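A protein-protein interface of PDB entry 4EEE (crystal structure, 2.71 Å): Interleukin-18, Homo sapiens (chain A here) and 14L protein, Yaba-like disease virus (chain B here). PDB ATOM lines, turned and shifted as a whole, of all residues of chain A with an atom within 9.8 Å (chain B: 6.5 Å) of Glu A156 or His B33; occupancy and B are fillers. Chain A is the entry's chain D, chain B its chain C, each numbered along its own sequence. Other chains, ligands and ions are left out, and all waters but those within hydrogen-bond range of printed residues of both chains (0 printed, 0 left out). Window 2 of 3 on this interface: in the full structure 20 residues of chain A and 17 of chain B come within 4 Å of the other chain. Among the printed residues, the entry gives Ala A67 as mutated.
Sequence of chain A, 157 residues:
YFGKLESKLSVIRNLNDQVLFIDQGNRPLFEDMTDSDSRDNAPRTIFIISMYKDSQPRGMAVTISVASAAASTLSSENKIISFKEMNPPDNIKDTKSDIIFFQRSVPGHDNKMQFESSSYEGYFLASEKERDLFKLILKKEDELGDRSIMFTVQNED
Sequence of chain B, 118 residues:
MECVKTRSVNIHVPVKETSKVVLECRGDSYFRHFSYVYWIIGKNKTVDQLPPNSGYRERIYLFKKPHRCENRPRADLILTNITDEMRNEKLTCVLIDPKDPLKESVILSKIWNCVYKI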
ATOM      1  N   LEU A   5     -17.346  -4.683  30.352  1.00  0.00           N
ATOM      2  CA  LEU A   5     -16.450  -3.576  30.660  1.00  0.00           C
ATOM      3  C   LEU A   5     -17.130  -2.252  31.014  1.00  0.00           C
ATOM      4  O   LEU A   5     -17.404  -1.972  32.179  1.00  0.00           O
ATOM      5  CB  LEU A   5     -15.473  -3.347  29.506  1.00  0.00           C
ATOM      6  CG  LEU A   5     -14.430  -4.441  29.275  1.00  0.00           C
ATOM      7  CD1 LEU A   5     -13.672  -4.197  27.979  1.00  0.00           C
ATOM      8  CD2 LEU A   5     -13.469  -4.533  30.450  1.00  0.00           C
ATOM      9  N   GLU A   6     -17.392  -1.447  29.993  1.00  0.00           N
ATOM     10  CA  GLU A   6     -17.836  -0.077  30.152  1.00  0.00           C
ATOM     11  C   GLU A   6     -19.210  -0.038  29.523  1.00  0.00           C
ATOM     12  O   GLU A   6     -19.532  -0.865  28.673  1.00  0.00           O
ATOM     13  CB  GLU A   6     -16.902   0.909  29.454  1.00  0.00           C
ATOM     14  CG  GLU A   6     -15.636   1.220  30.231  1.00  0.00           C
ATOM     15  CD  GLU A   6     -15.680   2.581  30.894  1.00  0.00           C
ATOM     16  N   SER A   7     -20.030   0.912  29.943  1.00  0.00           N
ATOM     17  CA  SER A   7     -21.407   0.936  29.498  1.00  0.00           C
ATOM     18  C   SER A   7     -21.790   2.393  29.134  1.00  0.00           C
ATOM     19  O   SER A   7     -21.344   3.338  29.786  1.00  0.00           O
ATOM     20  CB  SER A   7     -22.412   0.400  30.525  1.00  0.00           C
ATOM     21  OG  SER A   7     -21.990  -0.850  31.036  1.00  0.00           O
ATOM     22  N   LYS A   8     -22.612   2.563  28.101  1.00  0.00           N
ATOM     23  CA  LYS A   8     -22.948   3.897  27.606  1.00  0.00           C
ATOM     24  C   LYS A   8     -24.445   4.164  27.432  1.00  0.00           C
ATOM     25  O   LYS A   8     -25.152   3.411  26.756  1.00  0.00           O
ATOM     26  CB  LYS A   8     -22.242   4.142  26.260  1.00  0.00           C
ATOM     27  CG  LYS A   8     -20.727   4.272  26.349  1.00  0.00           C
ATOM     28  CD  LYS A   8     -20.295   5.722  26.551  1.00  0.00           C
ATOM     29  CE  LYS A   8     -18.777   5.869  26.531  1.00  0.00           C
ATOM     30  NZ  LYS A   8     -18.119   5.154  27.666  1.00  0.00           N
ATOM     31  N   LEU A   9     -24.914   5.264  28.015  1.00  0.00           N
ATOM     32  CA  LEU A   9     -26.264   5.743  27.759  1.00  0.00           C
ATOM     33  C   LEU A   9     -26.331   6.139  26.291  1.00  0.00           C
ATOM     34  O   LEU A   9     -25.518   6.937  25.821  1.00  0.00           O
ATOM     35  CB  LEU A   9     -26.592   6.941  28.650  1.00  0.00           C
ATOM     36  CG  LEU A   9     -26.731   6.656  30.147  1.00  0.00           C
ATOM     37  CD1 LEU A   9     -27.060   7.931  30.909  1.00  0.00           C
ATOM     38  CD2 LEU A   9     -27.789   5.592  30.395  1.00  0.00           C
ATOM     39  N   SER A  10     -27.286   5.573  25.562  1.00  0.00           N
ATOM     40  CA  SER A  10     -27.316   5.723  24.111  1.00  0.00           C
ATOM     41  C   SER A  10     -28.735   5.912  23.579  1.00  0.00           C
ATOM     42  O   SER A  10     -29.684   5.323  24.101  1.00  0.00           O
ATOM     43  CB  SER A  10     -26.681   4.495  23.445  1.00  0.00           C
ATOM     44  OG  SER A  10     -25.420   4.205  24.008  1.00  0.00           O
ATOM     45  N   VAL A  11     -28.875   6.742  22.547  1.00  0.00           N
ATOM     46  CA  VAL A  11     -30.126   6.825  21.788  1.00  0.00           C
ATOM     47  C   VAL A  11     -29.904   6.267  20.389  1.00  0.00           C
ATOM     48  O   VAL A  11     -28.972   6.673  19.693  1.00  0.00           O
ATOM     49  CB  VAL A  11     -30.667   8.265  21.680  1.00  0.00           C
ATOM     50  CG1 VAL A  11     -31.946   8.278  20.856  1.00  0.00           C
ATOM     51  CG2 VAL A  11     -30.917   8.850  23.054  1.00  0.00           C
ATOM     52  N   ILE A  46     -34.364   5.642  26.008  1.00  0.00           N
ATOM     53  CA  ILE A  46     -32.938   5.610  26.301  1.00  0.00           C
ATOM     54  C   ILE A  46     -32.451   4.206  26.658  1.00  0.00           C
ATOM     55  O   ILE A  46     -33.071   3.501  27.457  1.00  0.00           O
ATOM     56  CB  ILE A  46     -32.601   6.594  27.432  1.00  0.00           C
ATOM     57  CG1 ILE A  46     -32.947   8.024  26.995  1.00  0.00           C
ATOM     58  CG2 ILE A  46     -31.139   6.475  27.823  1.00  0.00           C
ATOM     59  CD1 ILE A  46     -32.999   9.029  28.135  1.00  0.00           C
ATOM     60  N   PHE A  47     -31.342   3.810  26.038  1.00  0.00           N
ATOM     61  CA  PHE A  47     -30.776   2.472  26.202  1.00  0.00           C
ATOM     62  C   PHE A  47     -29.352   2.511  26.745  1.00  0.00           C
ATOM     63  O   PHE A  47     -28.678   3.542  26.695  1.00  0.00           O
ATOM     64  CB  PHE A  47     -30.778   1.734  24.863  1.00  0.00           C
ATOM     65  CG  PHE A  47     -32.142   1.340  24.391  1.00  0.00           C
ATOM     66  CD1 PHE A  47     -32.575   0.030  24.524  1.00  0.00           C
ATOM     67  CD2 PHE A  47     -32.997   2.274  23.811  1.00  0.00           C
ATOM     68  CE1 PHE A  47     -33.838  -0.351  24.087  1.00  0.00           C
ATOM     69  CE2 PHE A  47     -34.267   1.903  23.370  1.00  0.00           C
ATOM     70  CZ  PHE A  47     -34.687   0.588  23.508  1.00  0.00           C
ATOM     71  N   ILE A  48     -28.896   1.373  27.256  1.00  0.00           N
ATOM     72  CA  ILE A  48     -27.513   1.236  27.698  1.00  0.00           C
ATOM     73  C   ILE A  48     -26.788   0.186  26.873  1.00  0.00           C
ATOM     74  O   ILE A  48     -27.058  -1.018  26.997  1.00  0.00           O
ATOM     75  CB  ILE A  48     -27.419   0.816  29.175  1.00  0.00           C
ATOM     76  CG1 ILE A  48     -28.043   1.886  30.078  1.00  0.00           C
ATOM     77  CG2 ILE A  48     -25.968   0.535  29.544  1.00  0.00           C
ATOM     78  CD1 ILE A  48     -28.372   1.397  31.470  1.00  0.00           C
ATOM     79  N   ILE A  49     -25.867   0.643  26.031  1.00  0.00           N
ATOM     80  CA  ILE A  49     -24.959  -0.271  25.352  1.00  0.00           C
ATOM     81  C   ILE A  49     -23.785  -0.608  26.278  1.00  0.00           C
ATOM     82  O   ILE A  49     -23.075   0.283  26.751  1.00  0.00           O
ATOM     83  CB  ILE A  49     -24.442   0.312  24.034  1.00  0.00           C
ATOM     84  CG1 ILE A  49     -25.624   0.773  23.175  1.00  0.00           C
ATOM     85  CG2 ILE A  49     -23.591  -0.710  23.302  1.00  0.00           C
ATOM     86  CD1 ILE A  49     -25.312   0.940  21.688  1.00  0.00           C
ATOM     87  N   SER A  50     -23.602  -1.897  26.553  1.00  0.00           N
ATOM     88  CA  SER A  50     -22.499  -2.339  27.398  1.00  0.00           C
ATOM     89  C   SER A  50     -21.462  -3.097  26.570  1.00  0.00           C
ATOM     90  O   SER A  50     -21.780  -4.089  25.904  1.00  0.00           O
ATOM     91  CB  SER A  50     -23.007  -3.210  28.554  1.00  0.00           C
ATOM     92  OG  SER A  50     -24.038  -2.543  29.261  1.00  0.00           O
ATOM     93  N   MET A  51     -20.224  -2.617  26.609  1.00  0.00           N
ATOM     94  CA  MET A  51     -19.137  -3.240  25.863  1.00  0.00           C
ATOM     95  C   MET A  51     -18.567  -4.429  26.623  1.00  0.00           C
ATOM     96  O   MET A  51     -18.490  -4.409  27.848  1.00  0.00           O
ATOM     97  CB  MET A  51     -18.041  -2.212  25.578  1.00  0.00           C
ATOM     98  CG  MET A  51     -18.467  -1.140  24.591  1.00  0.00           C
ATOM     99  SD  MET A  51     -17.374   0.295  24.560  1.00  0.00           S
ATOM    100  CE  MET A  51     -18.161   1.376  25.760  1.00  0.00           C
ATOM    101  N   MET A  60     -16.869  -5.615  18.177  1.00  0.00           N
ATOM    102  CA  MET A  60     -17.213  -5.039  19.470  1.00  0.00           C
ATOM    103  C   MET A  60     -18.459  -5.672  20.095  1.00  0.00           C
ATOM    104  O   MET A  60     -19.593  -5.281  19.799  1.00  0.00           O
ATOM    105  CB  MET A  60     -17.361  -3.521  19.382  1.00  0.00           C
ATOM    106  CG  MET A  60     -17.419  -2.856  20.734  1.00  0.00           C
ATOM    107  SD  MET A  60     -17.444  -1.065  20.601  1.00  0.00           S
ATOM    108  CE  MET A  60     -18.998  -0.830  19.720  1.00  0.00           C
ATOM    109  N   VAL A  62     -21.319  -6.218  22.377  1.00  0.00           N
ATOM    110  CA  VAL A  62     -22.132  -5.343  23.211  1.00  0.00           C
ATOM    111  C   VAL A  62     -23.454  -5.999  23.588  1.00  0.00           C
ATOM    112  O   VAL A  62     -23.935  -6.901  22.899  1.00  0.00           O
ATOM    113  CB  VAL A  62     -22.447  -4.013  22.507  1.00  0.00           C
ATOM    114  CG1 VAL A  62     -21.168  -3.351  22.014  1.00  0.00           C
ATOM    115  CG2 VAL A  62     -23.415  -4.247  21.343  1.00  0.00           C
ATOM    116  N   ALA A  67     -32.288   1.620  29.836  1.00  0.00           N
ATOM    117  CA  ALA A  67     -31.784   2.413  30.961  1.00  0.00           C
ATOM    118  C   ALA A  67     -33.072   2.678  31.736  1.00  0.00           C
ATOM    119  O   ALA A  67     -33.501   3.819  31.866  1.00  0.00           O
ATOM    120  CB  ALA A  67     -31.227   3.743  30.467  1.00  0.00           C
ATOM    121  N   GLN A 103     -21.203  -4.920  17.437  1.00  0.00           N
ATOM    122  CA  GLN A 103     -21.553  -3.588  16.939  1.00  0.00           C
ATOM    123  C   GLN A 103     -20.506  -3.129  15.945  1.00  0.00           C
ATOM    124  O   GLN A 103     -19.399  -2.737  16.322  1.00  0.00           O
ATOM    125  CB  GLN A 103     -21.673  -2.583  18.081  1.00  0.00           C
ATOM    126  CG  GLN A 103     -21.927  -1.169  17.607  1.00  0.00           C
ATOM    127  CD  GLN A 103     -22.102  -0.210  18.756  1.00  0.00           C
ATOM    128  OE1 GLN A 103     -22.586  -0.598  19.825  1.00  0.00           O
ATOM    129  NE2 GLN A 103     -21.698   1.050  18.555  1.00  0.00           N
ATOM    130  N   MET A 113     -23.974   2.253  12.303  1.00  0.00           N
ATOM    131  CA  MET A 113     -23.691   0.991  12.980  1.00  0.00           C
ATOM    132  C   MET A 113     -24.662  -0.135  12.626  1.00  0.00           C
ATOM    133  O   MET A 113     -25.858   0.090  12.460  1.00  0.00           O
ATOM    134  CB  MET A 113     -23.712   1.206  14.502  1.00  0.00           C
ATOM    135  CG  MET A 113     -22.742   2.260  14.976  1.00  0.00           C
ATOM    136  SD  MET A 113     -21.042   1.695  14.861  1.00  0.00           S
ATOM    137  CE  MET A 113     -20.201   3.250  14.548  1.00  0.00           C
ATOM    138  N   VAL A 153     -26.069   5.837  16.529  1.00  0.00           N
ATOM    139  CA  VAL A 153     -26.079   5.783  17.981  1.00  0.00           C
ATOM    140  C   VAL A 153     -25.603   7.120  18.500  1.00  0.00           C
ATOM    141  O   VAL A 153     -24.569   7.628  18.064  1.00  0.00           O
ATOM    142  CB  VAL A 153     -25.173   4.672  18.538  1.00  0.00           C
ATOM    143  CG1 VAL A 153     -25.449   4.475  20.023  1.00  0.00           C
ATOM    144  CG2 VAL A 153     -25.385   3.370  17.775  1.00  0.00           C
ATOM    145  N   GLN A 154     -26.365   7.693  19.425  1.00  0.00           N
ATOM    146  CA  GLN A 154     -26.057   9.010  19.962  1.00  0.00           C
ATOM    147  C   GLN A 154     -25.601   8.925  21.416  1.00  0.00           C
ATOM    148  O   GLN A 154     -26.189   8.207  22.223  1.00  0.00           O
ATOM    149  CB  GLN A 154     -27.293   9.889  19.859  1.00  0.00           C
ATOM    150  CG  GLN A 154     -27.018  11.354  20.086  1.00  0.00           C
ATOM    151  CD  GLN A 154     -28.165  12.041  20.801  1.00  0.00           C
ATOM    152  OE1 GLN A 154     -29.324  11.682  20.632  1.00  0.00           O
ATOM    153  NE2 GLN A 154     -27.843  13.020  21.614  1.00  0.00           N
ATOM    154  N   ASN A 155     -24.579   9.685  21.774  1.00  0.00           N
ATOM    155  CA  ASN A 155     -24.090   9.613  23.145  1.00  0.00           C
ATOM    156  C   ASN A 155     -23.818  10.970  23.796  1.00  0.00           C
ATOM    157  O   ASN A 155     -23.939  12.019  23.156  1.00  0.00           O
ATOM    158  CB  ASN A 155     -22.850   8.721  23.211  1.00  0.00           C
ATOM    159  CG  ASN A 155     -23.056   7.379  22.523  1.00  0.00           C
ATOM    160  OD1 ASN A 155     -22.431   7.087  21.498  1.00  0.00           O
ATOM    161  ND2 ASN A 155     -23.950   6.565  23.071  1.00  0.00           N
ATOM    162  N   GLU A 156     -23.462  10.943  25.078  1.00  0.00           N
ATOM    163  CA  GLU A 156     -23.253  12.173  25.837  1.00  0.00           C
ATOM    164  C   GLU A 156     -21.813  12.663  25.709  1.00  0.00           C
ATOM    165  O   GLU A 156     -21.550  13.677  25.059  1.00  0.00           O
ATOM    166  CB  GLU A 156     -23.626  11.966  27.312  1.00  0.00           C
ATOM    167  CG  GLU A 156     -24.809  11.031  27.520  1.00  0.00           C
ATOM    168  CD  GLU A 156     -25.249  10.944  28.970  1.00  0.00           C
ATOM    169  OE1 GLU A 156     -25.072  11.932  29.716  1.00  0.00           O
ATOM    170  OE2 GLU A 156     -25.778   9.885  29.364  1.00  0.00           O
ATOM    171  N   TYR B  30     -10.665   7.085  17.093  1.00  0.00           N
ATOM    172  CA  TYR B  30     -11.538   8.261  17.003  1.00  0.00           C
ATOM    173  C   TYR B  30     -12.974   7.937  17.407  1.00  0.00           C
ATOM    174  O   TYR B  30     -13.804   8.832  17.546  1.00  0.00           O
ATOM    175  CB  TYR B  30     -11.496   8.896  15.614  1.00  0.00           C
ATOM    176  CG  TYR B  30     -11.845   7.953  14.488  1.00  0.00           C
ATOM    177  CD1 TYR B  30     -10.867   7.183  13.881  1.00  0.00           C
ATOM    178  CD2 TYR B  30     -13.152   7.829  14.034  1.00  0.00           C
ATOM    179  CE1 TYR B  30     -11.174   6.313  12.856  1.00  0.00           C
ATOM    180  CE2 TYR B  30     -13.472   6.959  13.005  1.00  0.00           C
ATOM    181  CZ  TYR B  30     -12.477   6.203  12.419  1.00  0.00           C
ATOM    182  OH  TYR B  30     -12.773   5.335  11.391  1.00  0.00           O
ATOM    183  N   PHE B  31     -13.257   6.655  17.611  1.00  0.00           N
ATOM    184  CA  PHE B  31     -14.522   6.242  18.213  1.00  0.00           C
ATOM    185  C   PHE B  31     -14.502   6.517  19.712  1.00  0.00           C
ATOM    186  O   PHE B  31     -14.413   5.592  20.522  1.00  0.00           O
ATOM    187  CB  PHE B  31     -14.791   4.766  17.947  1.00  0.00           C
ATOM    188  CG  PHE B  31     -15.098   4.461  16.509  1.00  0.00           C
ATOM    189  CD1 PHE B  31     -16.339   4.768  15.968  1.00  0.00           C
ATOM    190  CD2 PHE B  31     -14.147   3.868  15.695  1.00  0.00           C
ATOM    191  CE1 PHE B  31     -16.622   4.486  14.641  1.00  0.00           C
ATOM    192  CE2 PHE B  31     -14.424   3.586  14.370  1.00  0.00           C
ATOM    193  CZ  PHE B  31     -15.663   3.896  13.842  1.00  0.00           C
ATOM    194  N   ARG B  32     -14.614   7.797  20.057  1.00  0.00           N
ATOM    195  CA  ARG B  32     -14.427   8.288  21.419  1.00  0.00           C
ATOM    196  C   ARG B  32     -15.186   7.522  22.511  1.00  0.00           C
ATOM    197  O   ARG B  32     -14.668   7.327  23.608  1.00  0.00           O
ATOM    198  CB  ARG B  32     -14.771   9.784  21.482  1.00  0.00           C
ATOM    199  CG  ARG B  32     -13.988  10.621  20.476  1.00  0.00           C
ATOM    200  CD  ARG B  32     -14.496  12.051  20.372  1.00  0.00           C
ATOM    201  NE  ARG B  32     -14.200  12.828  21.571  1.00  0.00           N
ATOM    202  CZ  ARG B  32     -15.101  13.152  22.492  1.00  0.00           C
ATOM    203  NH1 ARG B  32     -16.365  12.771  22.347  1.00  0.00           N
ATOM    204  NH2 ARG B  32     -14.741  13.863  23.552  1.00  0.00           N
ATOM    205  N   HIS B  33     -16.400   7.080  22.205  1.00  0.00           N
ATOM    206  CA  HIS B  33     -17.233   6.430  23.201  1.00  0.00           C
ATOM    207  C   HIS B  33     -17.208   4.927  23.145  1.00  0.00           C
ATOM    208  O   HIS B  33     -17.719   4.256  24.065  1.00  0.00           O
ATOM    209  CB  HIS B  33     -18.670   6.924  23.091  1.00  0.00           C
ATOM    210  CG  HIS B  33     -18.850   8.364  23.501  1.00  0.00           C
ATOM    211  ND1 HIS B  33     -19.303   9.305  22.655  1.00  0.00           N
ATOM    212  CD2 HIS B  33     -18.619   9.005  24.715  1.00  0.00           C
ATOM    213  CE1 HIS B  33     -19.360  10.489  23.293  1.00  0.00           C
ATOM    214  NE2 HIS B  33     -18.942  10.304  24.554  1.00  0.00           N
ATOM    215  N   PHE B  34     -16.628   4.369  22.089  1.00  0.00           N
ATOM    216  CA  PHE B  34     -16.652   2.926  21.898  1.00  0.00           C
ATOM    217  C   PHE B  34     -15.309   2.349  21.476  1.00  0.00           C
ATOM    218  O   PHE B  34     -15.186   1.738  20.414  1.00  0.00           O
ATOM    219  CB  PHE B  34     -17.720   2.540  20.877  1.00  0.00           C
ATOM    220  CG  PHE B  34     -19.120   2.788  21.344  1.00  0.00           C
ATOM    221  CD1 PHE B  34     -19.741   1.906  22.211  1.00  0.00           C
ATOM    222  CD2 PHE B  34     -19.815   3.909  20.925  1.00  0.00           C
ATOM    223  CE1 PHE B  34     -21.036   2.136  22.646  1.00  0.00           C
ATOM    224  CE2 PHE B  34     -21.109   4.146  21.355  1.00  0.00           C
ATOM    225  CZ  PHE B  34     -21.719   3.259  22.217  1.00  0.00           C
ATOM    226  N   SER B  35     -14.306   2.533  22.325  1.00  0.00           N
ATOM    227  CA  SER B  35     -12.994   1.961  22.081  1.00  0.00           C
ATOM    228  C   SER B  35     -12.340   1.567  23.401  1.00  0.00           C
ATOM    229  O   SER B  35     -12.422   2.294  24.394  1.00  0.00           O
ATOM    230  CB  SER B  35     -12.122   2.942  21.297  1.00  0.00           C
ATOM    231  OG  SER B  35     -12.121   4.229  21.908  1.00  0.00           O
ATOM    232  N   PRO B  66     -12.021  10.550  27.222  1.00  0.00           N
ATOM    233  CA  PRO B  66     -11.507  10.728  25.865  1.00  0.00           C
ATOM    234  C   PRO B  66     -11.082  12.172  25.649  1.00  0.00           C
ATOM    235  O   PRO B  66     -11.603  13.078  26.301  1.00  0.00           O
ATOM    236  CB  PRO B  66     -12.724  10.413  24.993  1.00  0.00           C
ATOM    237  CG  PRO B  66     -13.893  10.769  25.848  1.00  0.00           C
ATOM    238  CD  PRO B  66     -13.485  10.381  27.246  1.00  0.00           C
ATOM    239  N   ASN B  71     -10.278   8.652  21.710  1.00  0.00           N
ATOM    240  CA  ASN B  71     -10.185   8.013  23.007  1.00  0.00           C
ATOM    241  C   ASN B  71      -8.849   7.283  23.067  1.00  0.00           C
ATOM    242  O   ASN B  71      -8.426   6.668  22.084  1.00  0.00           O
ATOM    243  CB  ASN B  71     -11.340   7.037  23.224  1.00  0.00           C
ATOM    244  CG  ASN B  71     -11.335   6.445  24.618  1.00  0.00           C
ATOM    245  OD1 ASN B  71     -10.942   7.110  25.577  1.00  0.00           O
ATOM    246  ND2 ASN B  71     -11.755   5.186  24.739  1.00  0.00           N
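Of the 8 printed residues of chain B, 3 touch a printed residue of chain A. Of the 22 printed residues of chain A, 7 touch a printed residue of chain B. Among the printed residues, 9 pairs touch across the chains. Among the printed residues, no Asp or Glu carboxylate lies within 4 Å of a Lys or Arg side-chain nitrogen of the other chain.
Printed residues of chain B within 4 Å of Glu A156: His B33 (3.9 Å). His B33 touches just these residues of chain A: Lys A8 (3.1 Å), Met A51 (3.4 Å), Asn A155 (3.6 Å) and Glu A156 (3.9 Å). Of the printed residues of chain B, Asn A155 touches His B33 (3.6 Å) and Phe B34 (3.2 Å). Printed residues of chain B within 4 Å of Ile A49: Phe B34 (3.9 Å). Printed residues of chain B within 4 Å of Met A60: Phe B34. Of the printed residues of chain B, Met A113 touches Phe B31. Of the printed residues of chain B, Met A51 touches His B33 (3.4 Å) and Phe B34 (3.7 Å). Val A153 touches none of the printed residues of chain B. The nearest residue of chain B that does not touch Glu A156 is Arg B32 (5.9 Å). The nearest residue of chain A that does not touch His B33 is Met A60 (6.4 Å).
Among the printed residues, merely in contact across the chains: Lys A8 with His B33, Asn A155 with Phe B34, Met A51 with His B33, Asn A155 with His B33, Met A51 with Phe B34, Met A113 with Phe B31, Ile A49 with Phe B34 and Glu A156 with His B33.
The side-chain sulfur of Met A60 lies close to the backbone carbonyl oxygen of Phe B34, at 3.6 Å.
The side-chain hydroxyl (OG) of Ser B35 sits at hydrogen-bond distance from the backbone carbonyl oxygen (O) of Phe B31, at 3.0 Å. N of Leu A5 lies within hydrogen-bond range of O of Met A51 (2.8 Å). The backbone carbonyl oxygen of Lys A8 is in hydrogen-bond range of the side-chain hydroxyl of Ser A10 (2.9 Å). ND2 of Asn A155 sits at hydrogen-bond distance from O of Leu A9. The side-chain hydroxyl (OG) of Ser A10 is in hydrogen-bond range of the side-chain amide nitrogen (ND2) of Asn A155, at 2.9 Å. The backbone NH (N) of Gln A103 sits at hydrogen-bond distance from the backbone carbonyl oxygen (O) of Met A60, at 2.9 Å.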
